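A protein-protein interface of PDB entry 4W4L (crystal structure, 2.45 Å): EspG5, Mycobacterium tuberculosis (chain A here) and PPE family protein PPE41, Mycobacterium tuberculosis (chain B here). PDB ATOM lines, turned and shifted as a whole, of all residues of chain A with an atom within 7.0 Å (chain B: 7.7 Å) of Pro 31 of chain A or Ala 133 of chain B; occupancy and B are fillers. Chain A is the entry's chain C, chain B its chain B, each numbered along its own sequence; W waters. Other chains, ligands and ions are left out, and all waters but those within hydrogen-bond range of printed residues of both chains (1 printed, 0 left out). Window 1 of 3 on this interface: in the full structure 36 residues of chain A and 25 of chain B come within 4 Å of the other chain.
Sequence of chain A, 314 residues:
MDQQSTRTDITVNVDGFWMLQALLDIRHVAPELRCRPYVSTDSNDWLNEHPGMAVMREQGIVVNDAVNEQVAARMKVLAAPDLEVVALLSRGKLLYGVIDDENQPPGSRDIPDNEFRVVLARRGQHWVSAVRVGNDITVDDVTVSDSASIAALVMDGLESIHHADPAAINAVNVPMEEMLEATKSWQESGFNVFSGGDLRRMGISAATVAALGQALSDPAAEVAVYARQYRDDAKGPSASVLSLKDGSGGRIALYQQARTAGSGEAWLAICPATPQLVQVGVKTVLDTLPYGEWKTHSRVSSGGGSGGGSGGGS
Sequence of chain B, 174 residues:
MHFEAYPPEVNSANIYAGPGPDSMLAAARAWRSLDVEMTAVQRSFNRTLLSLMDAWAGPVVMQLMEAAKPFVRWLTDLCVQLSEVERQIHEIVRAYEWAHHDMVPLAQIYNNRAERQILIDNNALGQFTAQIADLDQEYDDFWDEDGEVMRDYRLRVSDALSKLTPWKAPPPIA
Water W1 lies within hydrogen-bond range of NH2 of Arg 109 of chain A (3.1 Å) and OD1 of Asp 140 of chain B (3.3 Å).
Of the 17 printed residues of chain B, 6 touch a printed residue of chain A. Hydrophobic or aromatic side chains of chain B within 4 Å of the printed part of chain A: Ala 130 and Ala 133. Hydrophobic or aromatic side chains of chain A that line the printed part of chain B: His 28, Pro 31, Leu 88 and Tyr 226. Among the printed residues, Asp or Glu carboxylates within 4 Å of a Lys or Arg side-chain nitrogen of the other chain: Arg 109 of chain A with Asp 140 of chain B (3.5 Å).
NE of Arg 116 of chain B is in salt-bridge range of OD1 of Asp 136 of chain B (2.6 Å). The backbone carbonyl oxygen of Cys 35 of chain A sits at hydrogen-bond distance from the guanidinium group of Arg 109 of chain A, at 2.7 Å. NH1 of Arg 228 of chain A lies within salt-bridge range of OE2 of Glu 32 of chain A (2.8 Å). The side-chain carboxylate (OE1) of Glu 84 of chain A is in salt-bridge range of the guanidinium group (NE) of Arg 228 of chain A, at 2.8 Å. NE of Arg 228 of chain A lies within hydrogen-bond range of OH of Tyr 230 of chain A (3.3 Å).
Of the printed residues of chain B, His 28 of chain A touches Gln 137 (3.7 Å). No residue of chain B comes within 4 Å of Ala 30 of chain A. Pro 31 of chain A touches three residues of chain B. Of the printed residues of chain B, Leu 88 of chain A touches Thr 129 (3.9 Å). Of the printed residues of chain B, Tyr 226 of chain A touches Thr 129, Ala 130 and Ala 133. Printed residues of chain A within 4 Å of Thr 129 of chain B: Leu 88 (3.9 Å) and Tyr 226 (3.5 Å). Ile 132 of chain B touches none of the printed residues of chain A. Of chain A, only Pro 31 (3.8 Å), Glu 32 (3.3 Å), Tyr 226 (3.4 Å) and Arg 228 (3.8 Å) come within 4 Å of Ala 133 of chain B. Asp 136 of chain B touches none of the printed residues of chain A. The nearest residue of chain B that does not touch Pro 31 of chain A is Asp 136 of chain B (4.04 Å).
His 28 of chain A touches Gln 137 of chain B (CD2 to NE2, 3.7 Å). Val 29 of chain A touches Gln 137 of chain B (O to OE1, 3.8 Å). O of Ala 133 of chain B touches CG of Pro 31 of chain A, at 3.8 Å. Pro 31 of chain A touches Gln 137 of chain B (CD to OE1, 3.3 Å). Asp 140 of chain B touches Pro 31 of chain A. OE2 of Glu 32 of chain A touches CB of Ala 133 of chain B (3.3 Å). Thr 129 of chain B touches Leu 88 of chain A (CG2 to CD1, 3.9 Å). CE1 of Tyr 226 of chain A touches CG2 of Thr 129 of chain B (3.5 Å). CB of Ala 133 of chain B touches OH of Tyr 226 of chain A, at 3.4 Å. Arg 228 of chain A touches Ala 133 of chain B (NH1 to CB, 3.8 Å).
NH2 of Arg 116 of chain B sits close to NH2 of Arg 34 of chain A (3.4 Å). The side-chain carboxylate (OD1) of Asp 140 of chain B is in salt-bridge range of the guanidinium group (NH1) of Arg 109 of chain A (3.5 Å).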
ATOM      1  N   HIS A  28     -34.815 -18.645  16.705  1.00  0.00           N
ATOM      2  CA  HIS A  28     -33.849 -19.454  17.425  1.00  0.00           C
ATOM      3  C   HIS A  28     -34.094 -20.945  17.242  1.00  0.00           C
ATOM      4  O   HIS A  28     -35.183 -21.377  16.859  1.00  0.00           O
ATOM      5  CB  HIS A  28     -33.869 -19.104  18.916  1.00  0.00           C
ATOM      6  CG  HIS A  28     -35.194 -19.328  19.573  1.00  0.00           C
ATOM      7  ND1 HIS A  28     -36.298 -18.544  19.311  1.00  0.00           N
ATOM      8  CD2 HIS A  28     -35.593 -20.244  20.487  1.00  0.00           C
ATOM      9  CE1 HIS A  28     -37.320 -18.970  20.032  1.00  0.00           C
ATOM     10  NE2 HIS A  28     -36.919 -20.000  20.754  1.00  0.00           N
ATOM     11  N   VAL A  29     -33.054 -21.720  17.520  1.00  0.00           N
ATOM     12  CA  VAL A  29     -33.124 -23.171  17.542  1.00  0.00           C
ATOM     13  C   VAL A  29     -32.618 -23.620  18.904  1.00  0.00           C
ATOM     14  O   VAL A  29     -32.391 -22.789  19.782  1.00  0.00           O
ATOM     15  CB  VAL A  29     -32.289 -23.810  16.420  1.00  0.00           C
ATOM     16  CG1 VAL A  29     -32.915 -23.532  15.064  1.00  0.00           C
ATOM     17  CG2 VAL A  29     -30.858 -23.295  16.466  1.00  0.00           C
ATOM     18  N   ALA A  30     -32.452 -24.925  19.081  1.00  0.00           N
ATOM     19  CA  ALA A  30     -31.932 -25.468  20.333  1.00  0.00           C
ATOM     20  C   ALA A  30     -30.663 -24.738  20.772  1.00  0.00           C
ATOM     21  O   ALA A  30     -29.765 -24.499  19.963  1.00  0.00           O
ATOM     22  CB  ALA A  30     -31.658 -26.960  20.187  1.00  0.00           C
ATOM     23  N   PRO A  31     -30.604 -24.351  22.054  1.00  0.00           N
ATOM     24  CA  PRO A  31     -29.434 -23.678  22.633  1.00  0.00           C
ATOM     25  C   PRO A  31     -28.168 -24.524  22.569  1.00  0.00           C
ATOM     26  O   PRO A  31     -27.062 -23.986  22.627  1.00  0.00           O
ATOM     27  CB  PRO A  31     -29.850 -23.435  24.091  1.00  0.00           C
ATOM     28  CG  PRO A  31     -30.985 -24.378  24.339  1.00  0.00           C
ATOM     29  CD  PRO A  31     -31.699 -24.489  23.029  1.00  0.00           C
ATOM     30  N   GLU A  32     -28.330 -25.836  22.452  1.00  0.00           N
ATOM     31  CA  GLU A  32     -27.184 -26.730  22.407  1.00  0.00           C
ATOM     32  C   GLU A  32     -26.406 -26.564  21.109  1.00  0.00           C
ATOM     33  O   GLU A  32     -25.206 -26.826  21.061  1.00  0.00           O
ATOM     34  CB  GLU A  32     -27.625 -28.181  22.577  1.00  0.00           C
ATOM     35  CG  GLU A  32     -28.202 -28.486  23.944  1.00  0.00           C
ATOM     36  CD  GLU A  32     -29.675 -28.152  24.049  1.00  0.00           C
ATOM     37  OE1 GLU A  32     -30.266 -27.739  23.028  1.00  0.00           O
ATOM     38  OE2 GLU A  32     -30.241 -28.307  25.151  1.00  0.00           O
ATOM     39  N   LEU A  33     -27.092 -26.127  20.057  1.00  0.00           N
ATOM     40  CA  LEU A  33     -26.432 -25.849  18.787  1.00  0.00           C
ATOM     41  C   LEU A  33     -25.608 -24.576  18.905  1.00  0.00           C
ATOM     42  O   LEU A  33     -24.654 -24.368  18.153  1.00  0.00           O
ATOM     43  CB  LEU A  33     -27.454 -25.725  17.659  1.00  0.00           C
ATOM     44  CG  LEU A  33     -28.201 -27.014  17.316  1.00  0.00           C
ATOM     45  CD1 LEU A  33     -29.056 -26.831  16.070  1.00  0.00           C
ATOM     46  CD2 LEU A  33     -27.218 -28.169  17.142  1.00  0.00           C
ATOM     47  N   ARG A  34     -26.001 -23.736  19.858  1.00  0.00           N
ATOM     48  CA  ARG A  34     -25.288 -22.512  20.207  1.00  0.00           C
ATOM     49  C   ARG A  34     -25.053 -21.592  19.005  1.00  0.00           C
ATOM     50  O   ARG A  34     -23.916 -21.230  18.699  1.00  0.00           O
ATOM     51  CB  ARG A  34     -23.961 -22.850  20.891  1.00  0.00           C
ATOM     52  CG  ARG A  34     -23.383 -21.709  21.712  1.00  0.00           C
ATOM     53  CD  ARG A  34     -22.230 -22.168  22.586  1.00  0.00           C
ATOM     54  NE  ARG A  34     -22.662 -22.439  23.953  1.00  0.00           N
ATOM     55  CZ  ARG A  34     -21.841 -22.770  24.944  1.00  0.00           C
ATOM     56  NH1 ARG A  34     -20.536 -22.878  24.724  1.00  0.00           N
ATOM     57  NH2 ARG A  34     -22.325 -22.997  26.158  1.00  0.00           N
ATOM     58  N   CYS A  35     -26.131 -21.234  18.312  1.00  0.00           N
ATOM     59  CA  CYS A  35     -26.050 -20.203  17.286  1.00  0.00           C
ATOM     60  C   CYS A  35     -26.440 -18.857  17.873  1.00  0.00           C
ATOM     61  O   CYS A  35     -26.869 -18.775  19.025  1.00  0.00           O
ATOM     62  CB  CYS A  35     -26.960 -20.540  16.106  1.00  0.00           C
ATOM     63  SG  CYS A  35     -26.595 -22.124  15.334  1.00  0.00           S
ATOM     64  N   GLU A  84     -37.826 -32.434  21.509  1.00  0.00           N
ATOM     65  CA  GLU A  84     -36.381 -32.340  21.329  1.00  0.00           C
ATOM     66  C   GLU A  84     -35.668 -33.377  22.184  1.00  0.00           C
ATOM     67  O   GLU A  84     -36.045 -33.620  23.326  1.00  0.00           O
ATOM     68  CB  GLU A  84     -35.876 -30.937  21.667  1.00  0.00           C
ATOM     69  CG  GLU A  84     -36.052 -29.929  20.542  1.00  0.00           C
ATOM     70  CD  GLU A  84     -35.690 -28.514  20.957  1.00  0.00           C
ATOM     71  OE1 GLU A  84     -35.763 -28.208  22.166  1.00  0.00           O
ATOM     72  OE2 GLU A  84     -35.330 -27.707  20.075  1.00  0.00           O
ATOM     73  N   VAL A  86     -31.685 -34.264  23.232  1.00  0.00           N
ATOM     74  CA  VAL A  86     -30.320 -33.768  23.191  1.00  0.00           C
ATOM     75  C   VAL A  86     -29.324 -34.762  23.785  1.00  0.00           C
ATOM     76  O   VAL A  86     -29.600 -35.402  24.808  1.00  0.00           O
ATOM     77  CB  VAL A  86     -30.209 -32.429  23.947  1.00  0.00           C
ATOM     78  CG1 VAL A  86     -28.760 -31.971  24.027  1.00  0.00           C
ATOM     79  CG2 VAL A  86     -31.074 -31.373  23.280  1.00  0.00           C
ATOM     80  N   LEU A  88     -25.122 -34.573  24.738  1.00  0.00           N
ATOM     81  CA  LEU A  88     -23.836 -33.888  24.789  1.00  0.00           C
ATOM     82  C   LEU A  88     -22.723 -34.913  24.945  1.00  0.00           C
ATOM     83  O   LEU A  88     -22.658 -35.611  25.952  1.00  0.00           O
ATOM     84  CB  LEU A  88     -23.787 -32.886  25.945  1.00  0.00           C
ATOM     85  CG  LEU A  88     -24.914 -31.859  26.080  1.00  0.00           C
ATOM     86  CD1 LEU A  88     -24.686 -30.990  27.312  1.00  0.00           C
ATOM     87  CD2 LEU A  88     -25.041 -31.002  24.827  1.00  0.00           C
ATOM     88  N   ARG A 109     -19.968 -18.179  20.887  1.00  0.00           N
ATOM     89  CA  ARG A 109     -20.718 -19.259  20.270  1.00  0.00           C
ATOM     90  C   ARG A 109     -19.837 -20.491  20.100  1.00  0.00           C
ATOM     91  O   ARG A 109     -20.280 -21.509  19.570  1.00  0.00           O
ATOM     92  CB  ARG A 109     -21.296 -18.813  18.925  1.00  0.00           C
ATOM     93  CG  ARG A 109     -22.176 -17.557  18.998  1.00  0.00           C
ATOM     94  CD  ARG A 109     -23.526 -17.821  19.667  1.00  0.00           C
ATOM     95  NE  ARG A 109     -23.453 -17.825  21.129  1.00  0.00           N
ATOM     96  CZ  ARG A 109     -24.468 -18.148  21.927  1.00  0.00           C
ATOM     97  NH1 ARG A 109     -25.638 -18.501  21.408  1.00  0.00           N
ATOM     98  NH2 ARG A 109     -24.313 -18.123  23.243  1.00  0.00           N
ATOM     99  N   ARG A 117     -22.278 -31.856  20.206  1.00  0.00           N
ATOM    100  CA  ARG A 117     -23.652 -32.022  20.668  1.00  0.00           C
ATOM    101  C   ARG A 117     -24.593 -32.422  19.542  1.00  0.00           C
ATOM    102  O   ARG A 117     -24.498 -31.915  18.433  1.00  0.00           O
ATOM    103  CB  ARG A 117     -24.149 -30.733  21.327  1.00  0.00           C
ATOM    104  CG  ARG A 117     -23.298 -29.513  21.020  1.00  0.00           C
ATOM    105  CD  ARG A 117     -22.560 -29.025  22.255  1.00  0.00           C
ATOM    106  NE  ARG A 117     -23.097 -27.754  22.720  1.00  0.00           N
ATOM    107  CZ  ARG A 117     -22.771 -27.173  23.868  1.00  0.00           C
ATOM    108  NH1 ARG A 117     -21.904 -27.750  24.682  1.00  0.00           N
ATOM    109  NH2 ARG A 117     -23.321 -26.016  24.202  1.00  0.00           N
ATOM    110  N   VAL A 119     -28.631 -32.843  18.414  1.00  0.00           N
ATOM    111  CA  VAL A 119     -30.024 -32.518  18.670  1.00  0.00           C
ATOM    112  C   VAL A 119     -30.938 -33.240  17.688  1.00  0.00           C
ATOM    113  O   VAL A 119     -30.899 -32.985  16.484  1.00  0.00           O
ATOM    114  CB  VAL A 119     -30.279 -31.004  18.568  1.00  0.00           C
ATOM    115  CG1 VAL A 119     -31.759 -30.706  18.747  1.00  0.00           C
ATOM    116  CG2 VAL A 119     -29.449 -30.256  19.599  1.00  0.00           C
ATOM    117  N   TYR A 226     -30.857 -35.878  27.443  1.00  0.00           N
ATOM    118  CA  TYR A 226     -32.055 -35.328  28.076  1.00  0.00           C
ATOM    119  C   TYR A 226     -33.013 -34.811  27.011  1.00  0.00           C
ATOM    120  O   TYR A 226     -32.625 -34.647  25.867  1.00  0.00           O
ATOM    121  CB  TYR A 226     -31.694 -34.213  29.058  1.00  0.00           C
ATOM    122  CG  TYR A 226     -30.951 -33.056  28.433  1.00  0.00           C
ATOM    123  CD1 TYR A 226     -29.575 -33.105  28.262  1.00  0.00           C
ATOM    124  CD2 TYR A 226     -31.622 -31.911  28.022  1.00  0.00           C
ATOM    125  CE1 TYR A 226     -28.887 -32.055  27.693  1.00  0.00           C
ATOM    126  CE2 TYR A 226     -30.940 -30.851  27.452  1.00  0.00           C
ATOM    127  CZ  TYR A 226     -29.571 -30.933  27.292  1.00  0.00           C
ATOM    128  OH  TYR A 226     -28.874 -29.891  26.726  1.00  0.00           O
ATOM    129  N   ARG A 228     -36.658 -32.263  25.789  1.00  0.00           N
ATOM    130  CA  ARG A 228     -37.518 -31.104  25.996  1.00  0.00           C
ATOM    131  C   ARG A 228     -38.838 -31.284  25.261  1.00  0.00           C
ATOM    132  O   ARG A 228     -38.877 -31.839  24.160  1.00  0.00           O
ATOM    133  CB  ARG A 228     -36.837 -29.820  25.516  1.00  0.00           C
ATOM    134  CG  ARG A 228     -36.129 -29.033  26.600  1.00  0.00           C
ATOM    135  CD  ARG A 228     -35.747 -27.651  26.094  1.00  0.00           C
ATOM    136  NE  ARG A 228     -35.006 -27.724  24.838  1.00  0.00           N
ATOM    137  CZ  ARG A 228     -33.689 -27.879  24.759  1.00  0.00           C
ATOM    138  NH1 ARG A 228     -32.966 -27.975  25.865  1.00  0.00           N
ATOM    139  NH2 ARG A 228     -33.094 -27.937  23.576  1.00  0.00           N
ATOM    140  N   TYR A 230     -42.578 -29.204  24.122  1.00  0.00           N
ATOM    141  CA  TYR A 230     -43.210 -27.904  23.941  1.00  0.00           C
ATOM    142  C   TYR A 230     -44.721 -28.037  23.837  1.00  0.00           C
ATOM    143  O   TYR A 230     -45.221 -28.929  23.153  1.00  0.00           O
ATOM    144  CB  TYR A 230     -42.663 -27.217  22.689  1.00  0.00           C
ATOM    145  CG  TYR A 230     -41.180 -26.932  22.741  1.00  0.00           C
ATOM    146  CD1 TYR A 230     -40.252 -27.922  22.440  1.00  0.00           C
ATOM    147  CD2 TYR A 230     -40.709 -25.674  23.086  1.00  0.00           C
ATOM    148  CE1 TYR A 230     -38.891 -27.665  22.486  1.00  0.00           C
ATOM    149  CE2 TYR A 230     -39.353 -25.404  23.135  1.00  0.00           C
ATOM    150  CZ  TYR A 230     -38.447 -26.404  22.834  1.00  0.00           C
ATOM    151  OH  TYR A 230     -37.098 -26.140  22.882  1.00  0.00           O
ATOM    152  N   ASN B 112     -28.160 -14.947  35.515  1.00  0.00           N
ATOM    153  CA  ASN B 112     -28.262 -16.112  34.655  1.00  0.00           C
ATOM    154  C   ASN B 112     -26.947 -16.889  34.611  1.00  0.00           C
ATOM    155  O   ASN B 112     -26.914 -18.089  34.924  1.00  0.00           O
ATOM    156  CB  ASN B 112     -28.681 -15.697  33.246  1.00  0.00           C
ATOM    157  CG  ASN B 112     -28.736 -16.869  32.290  1.00  0.00           C
ATOM    158  OD1 ASN B 112     -27.724 -17.249  31.703  1.00  0.00           O
ATOM    159  ND2 ASN B 112     -29.920 -17.451  32.130  1.00  0.00           N
ATOM    160  N   ARG B 113     -25.861 -16.200  34.260  1.00  0.00           N
ATOM    161  CA  ARG B 113     -24.562 -16.870  34.137  1.00  0.00           C
ATOM    162  C   ARG B 113     -24.100 -17.484  35.463  1.00  0.00           C
ATOM    163  O   ARG B 113     -23.540 -18.584  35.490  1.00  0.00           O
ATOM    164  CB  ARG B 113     -23.499 -15.897  33.617  1.00  0.00           C
ATOM    165  CG  ARG B 113     -23.828 -15.240  32.281  1.00  0.00           C
ATOM    166  CD  ARG B 113     -23.730 -16.205  31.100  1.00  0.00           C
ATOM    167  NE  ARG B 113     -24.890 -17.087  30.998  1.00  0.00           N
ATOM    168  CZ  ARG B 113     -24.973 -18.120  30.165  1.00  0.00           C
ATOM    169  NH1 ARG B 113     -23.962 -18.402  29.350  1.00  0.00           N
ATOM    170  NH2 ARG B 113     -26.065 -18.873  30.145  1.00  0.00           N
ATOM    171  N   ARG B 116     -26.056 -20.570  36.240  1.00  0.00           N
ATOM    172  CA  ARG B 116     -25.534 -21.592  35.338  1.00  0.00           C
ATOM    173  C   ARG B 116     -24.250 -22.210  35.894  1.00  0.00           C
ATOM    174  O   ARG B 116     -24.116 -23.435  35.953  1.00  0.00           O
ATOM    175  CB  ARG B 116     -25.275 -21.009  33.948  1.00  0.00           C
ATOM    176  CG  ARG B 116     -24.972 -22.056  32.884  1.00  0.00           C
ATOM    177  CD  ARG B 116     -24.181 -21.463  31.726  1.00  0.00           C
ATOM    178  NE  ARG B 116     -24.276 -22.280  30.521  1.00  0.00           N
ATOM    179  CZ  ARG B 116     -23.451 -23.277  30.225  1.00  0.00           C
ATOM    180  NH1 ARG B 116     -22.460 -23.587  31.051  1.00  0.00           N
ATOM    181  NH2 ARG B 116     -23.617 -23.968  29.104  1.00  0.00           N
ATOM    182  N   LEU B 119     -24.817 -24.453  38.840  1.00  0.00           N
ATOM    183  CA  LEU B 119     -25.301 -25.760  38.387  1.00  0.00           C
ATOM    184  C   LEU B 119     -24.161 -26.614  37.833  1.00  0.00           C
ATOM    185  O   LEU B 119     -24.084 -27.816  38.111  1.00  0.00           O
ATOM    186  CB  LEU B 119     -26.400 -25.605  37.335  1.00  0.00           C
ATOM    187  CG  LEU B 119     -27.703 -24.974  37.829  1.00  0.00           C
ATOM    188  CD1 LEU B 119     -28.801 -25.097  36.784  1.00  0.00           C
ATOM    189  CD2 LEU B 119     -28.139 -25.601  39.142  1.00  0.00           C
ATOM    190  N   PHE B 128     -28.298 -31.956  36.464  1.00  0.00           N
ATOM    191  CA  PHE B 128     -28.668 -30.550  36.309  1.00  0.00           C
ATOM    192  C   PHE B 128     -28.551 -30.065  34.866  1.00  0.00           C
ATOM    193  O   PHE B 128     -28.752 -28.885  34.584  1.00  0.00           O
ATOM    194  CB  PHE B 128     -27.815 -29.673  37.224  1.00  0.00           C
ATOM    195  CG  PHE B 128     -28.102 -29.872  38.681  1.00  0.00           C
ATOM    196  CD1 PHE B 128     -29.331 -29.513  39.210  1.00  0.00           C
ATOM    197  CD2 PHE B 128     -27.147 -30.414  39.523  1.00  0.00           C
ATOM    198  CE1 PHE B 128     -29.604 -29.694  40.552  1.00  0.00           C
ATOM    199  CE2 PHE B 128     -27.413 -30.598  40.869  1.00  0.00           C
ATOM    200  CZ  PHE B 128     -28.642 -30.239  41.383  1.00  0.00           C
ATOM    201  N   THR B 129     -28.218 -30.981  33.965  1.00  0.00           N
ATOM    202  CA  THR B 129     -27.854 -30.644  32.588  1.00  0.00           C
ATOM    203  C   THR B 129     -28.970 -29.932  31.819  1.00  0.00           C
ATOM    204  O   THR B 129     -28.737 -28.905  31.154  1.00  0.00           O
ATOM    205  CB  THR B 129     -27.435 -31.921  31.823  1.00  0.00           C
ATOM    206  OG1 THR B 129     -26.500 -32.665  32.616  1.00  0.00           O
ATOM    207  CG2 THR B 129     -26.797 -31.576  30.487  1.00  0.00           C
ATOM    208  N   ALA B 130     -30.181 -30.467  31.917  1.00  0.00           N
ATOM    209  CA  ALA B 130     -31.329 -29.863  31.253  1.00  0.00           C
ATOM    210  C   ALA B 130     -31.594 -28.452  31.783  1.00  0.00           C
ATOM    211  O   ALA B 130     -31.953 -27.554  31.024  1.00  0.00           O
ATOM    212  CB  ALA B 130     -32.559 -30.741  31.419  1.00  0.00           C
ATOM    213  N   GLN B 131     -31.405 -28.257  33.085  1.00  0.00           N
ATOM    214  CA  GLN B 131     -31.608 -26.943  33.687  1.00  0.00           C
ATOM    215  C   GLN B 131     -30.575 -25.948  33.161  1.00  0.00           C
ATOM    216  O   GLN B 131     -30.888 -24.783  32.907  1.00  0.00           O
ATOM    217  CB  GLN B 131     -31.539 -27.032  35.212  1.00  0.00           C
ATOM    218  CG  GLN B 131     -32.665 -27.852  35.823  1.00  0.00           C
ATOM    219  CD  GLN B 131     -32.603 -27.908  37.339  1.00  0.00           C
ATOM    220  OE1 GLN B 131     -31.894 -27.128  37.975  1.00  0.00           O
ATOM    221  NE2 GLN B 131     -33.346 -28.838  37.925  1.00  0.00           N
ATOM    222  N   ILE B 132     -29.348 -26.422  32.995  1.00  0.00           N
ATOM    223  CA  ILE B 132     -28.275 -25.629  32.409  1.00  0.00           C
ATOM    224  C   ILE B 132     -28.659 -25.199  30.997  1.00  0.00           C
ATOM    225  O   ILE B 132     -28.510 -24.023  30.622  1.00  0.00           O
ATOM    226  CB  ILE B 132     -26.952 -26.418  32.389  1.00  0.00           C
ATOM    227  CG1 ILE B 132     -26.498 -26.710  33.821  1.00  0.00           C
ATOM    228  CG2 ILE B 132     -25.879 -25.657  31.636  1.00  0.00           C
ATOM    229  CD1 ILE B 132     -25.399 -27.747  33.924  1.00  0.00           C
ATOM    230  N   ALA B 133     -29.182 -26.149  30.225  1.00  0.00           N
ATOM    231  CA  ALA B 133     -29.674 -25.840  28.886  1.00  0.00           C
ATOM    232  C   ALA B 133     -30.786 -24.787  28.930  1.00  0.00           C
ATOM    233  O   ALA B 133     -30.831 -23.890  28.083  1.00  0.00           O
ATOM    234  CB  ALA B 133     -30.161 -27.094  28.197  1.00  0.00           C
ATOM    235  N   ASP B 134     -31.675 -24.895  29.915  1.00  0.00           N
ATOM    236  CA  ASP B 134     -32.750 -23.916  30.089  1.00  0.00           C
ATOM    237  C   ASP B 134     -32.185 -22.523  30.331  1.00  0.00           C
ATOM    238  O   ASP B 134     -32.641 -21.546  29.738  1.00  0.00           O
ATOM    239  CB  ASP B 134     -33.668 -24.303  31.251  1.00  0.00           C
ATOM    240  CG  ASP B 134     -34.737 -25.296  30.850  1.00  0.00           C
ATOM    241  OD1 ASP B 134     -35.113 -25.318  29.659  1.00  0.00           O
ATOM    242  OD2 ASP B 134     -35.210 -26.049  31.732  1.00  0.00           O
ATOM    243  N   LEU B 135     -31.189 -22.440  31.208  1.00  0.00           N
ATOM    244  CA  LEU B 135     -30.536 -21.169  31.492  1.00  0.00           C
ATOM    245  C   LEU B 135     -29.889 -20.601  30.235  1.00  0.00           C
ATOM    246  O   LEU B 135     -29.925 -19.387  30.000  1.00  0.00           O
ATOM    247  CB  LEU B 135     -29.503 -21.338  32.602  1.00  0.00           C
ATOM    248  CG  LEU B 135     -30.141 -21.457  33.985  1.00  0.00           C
ATOM    249  CD1 LEU B 135     -29.135 -21.912  35.033  1.00  0.00           C
ATOM    250  CD2 LEU B 135     -30.749 -20.123  34.371  1.00  0.00           C
ATOM    251  N   ASP B 136     -29.311 -21.480  29.421  1.00  0.00           N
ATOM    252  CA  ASP B 136     -28.746 -21.054  28.144  1.00  0.00           C
ATOM    253  C   ASP B 136     -29.826 -20.499  27.208  1.00  0.00           C
ATOM    254  O   ASP B 136     -29.603 -19.516  26.487  1.00  0.00           O
ATOM    255  CB  ASP B 136     -28.005 -22.214  27.477  1.00  0.00           C
ATOM    256  CG  ASP B 136     -26.660 -22.489  28.121  1.00  0.00           C
ATOM    257  OD1 ASP B 136     -26.096 -21.563  28.741  1.00  0.00           O
ATOM    258  OD2 ASP B 136     -26.166 -23.629  28.004  1.00  0.00           O
ATOM    259  N   GLN B 137     -31.002 -21.117  27.223  1.00  0.00           N
ATOM    260  CA  GLN B 137     -32.101 -20.614  26.406  1.00  0.00           C
ATOM    261  C   GLN B 137     -32.580 -19.251  26.910  1.00  0.00           C
ATOM    262  O   GLN B 137     -32.936 -18.379  26.114  1.00  0.00           O
ATOM    263  CB  GLN B 137     -33.264 -21.608  26.379  1.00  0.00           C
ATOM    264  CG  GLN B 137     -34.400 -21.202  25.453  1.00  0.00           C
ATOM    265  CD  GLN B 137     -33.958 -21.019  24.005  1.00  0.00           C
ATOM    266  OE1 GLN B 137     -33.855 -21.986  23.250  1.00  0.00           O
ATOM    267  NE2 GLN B 137     -33.709 -19.773  23.611  1.00  0.00           N
ATOM    268  N   GLU B 138     -32.585 -19.066  28.227  1.00  0.00           N
ATOM    269  CA  GLU B 138     -32.957 -17.776  28.802  1.00  0.00           C
ATOM    270  C   GLU B 138     -31.956 -16.713  28.368  1.00  0.00           C
ATOM    271  O   GLU B 138     -32.338 -15.599  28.005  1.00  0.00           O
ATOM    272  CB  GLU B 138     -33.033 -17.847  30.330  1.00  0.00           C
ATOM    273  CG  GLU B 138     -33.524 -16.561  30.978  1.00  0.00           C
ATOM    274  CD  GLU B 138     -33.559 -16.625  32.498  1.00  0.00           C
ATOM    275  OE1 GLU B 138     -32.527 -16.975  33.115  1.00  0.00           O
ATOM    276  OE2 GLU B 138     -34.623 -16.314  33.077  1.00  0.00           O
ATOM    277  N   TYR B 139     -30.674 -17.066  28.394  1.00  0.00           N
ATOM    278  CA  TYR B 139     -29.626 -16.148  27.945  1.00  0.00           C
ATOM    279  C   TYR B 139     -29.813 -15.767  26.472  1.00  0.00           C
ATOM    280  O   TYR B 139     -29.671 -14.596  26.086  1.00  0.00           O
ATOM    281  CB  TYR B 139     -28.248 -16.773  28.169  1.00  0.00           C
ATOM    282  CG  TYR B 139     -27.090 -15.890  27.766  1.00  0.00           C
ATOM    283  CD1 TYR B 139     -26.577 -14.943  28.641  1.00  0.00           C
ATOM    284  CD2 TYR B 139     -26.501 -16.015  26.515  1.00  0.00           C
ATOM    285  CE1 TYR B 139     -25.513 -14.139  28.280  1.00  0.00           C
ATOM    286  CE2 TYR B 139     -25.441 -15.215  26.144  1.00  0.00           C
ATOM    287  CZ  TYR B 139     -24.951 -14.281  27.030  1.00  0.00           C
ATOM    288  OH  TYR B 139     -23.897 -13.481  26.661  1.00  0.00           O
ATOM    289  N   ASP B 140     -30.142 -16.760  25.650  1.00  0.00           N
ATOM    290  CA  ASP B 140     -30.430 -16.493  24.244  1.00  0.00           C
ATOM    291  C   ASP B 140     -31.656 -15.604  24.077  1.00  0.00           C
ATOM    292  O   ASP B 140     -31.748 -14.833  23.120  1.00  0.00           O
ATOM    293  CB  ASP B 140     -30.618 -17.803  23.477  1.00  0.00           C
ATOM    294  CG  ASP B 140     -29.322 -18.558  23.307  1.00  0.00           C
ATOM    295  OD1 ASP B 140     -28.262 -17.988  23.644  1.00  0.00           O
ATOM    296  OD2 ASP B 140     -29.357 -19.710  22.826  1.00  0.00           O
HETATM  297  O   HOH W   1     -25.945 -19.526  25.423  1.00  0.00           O
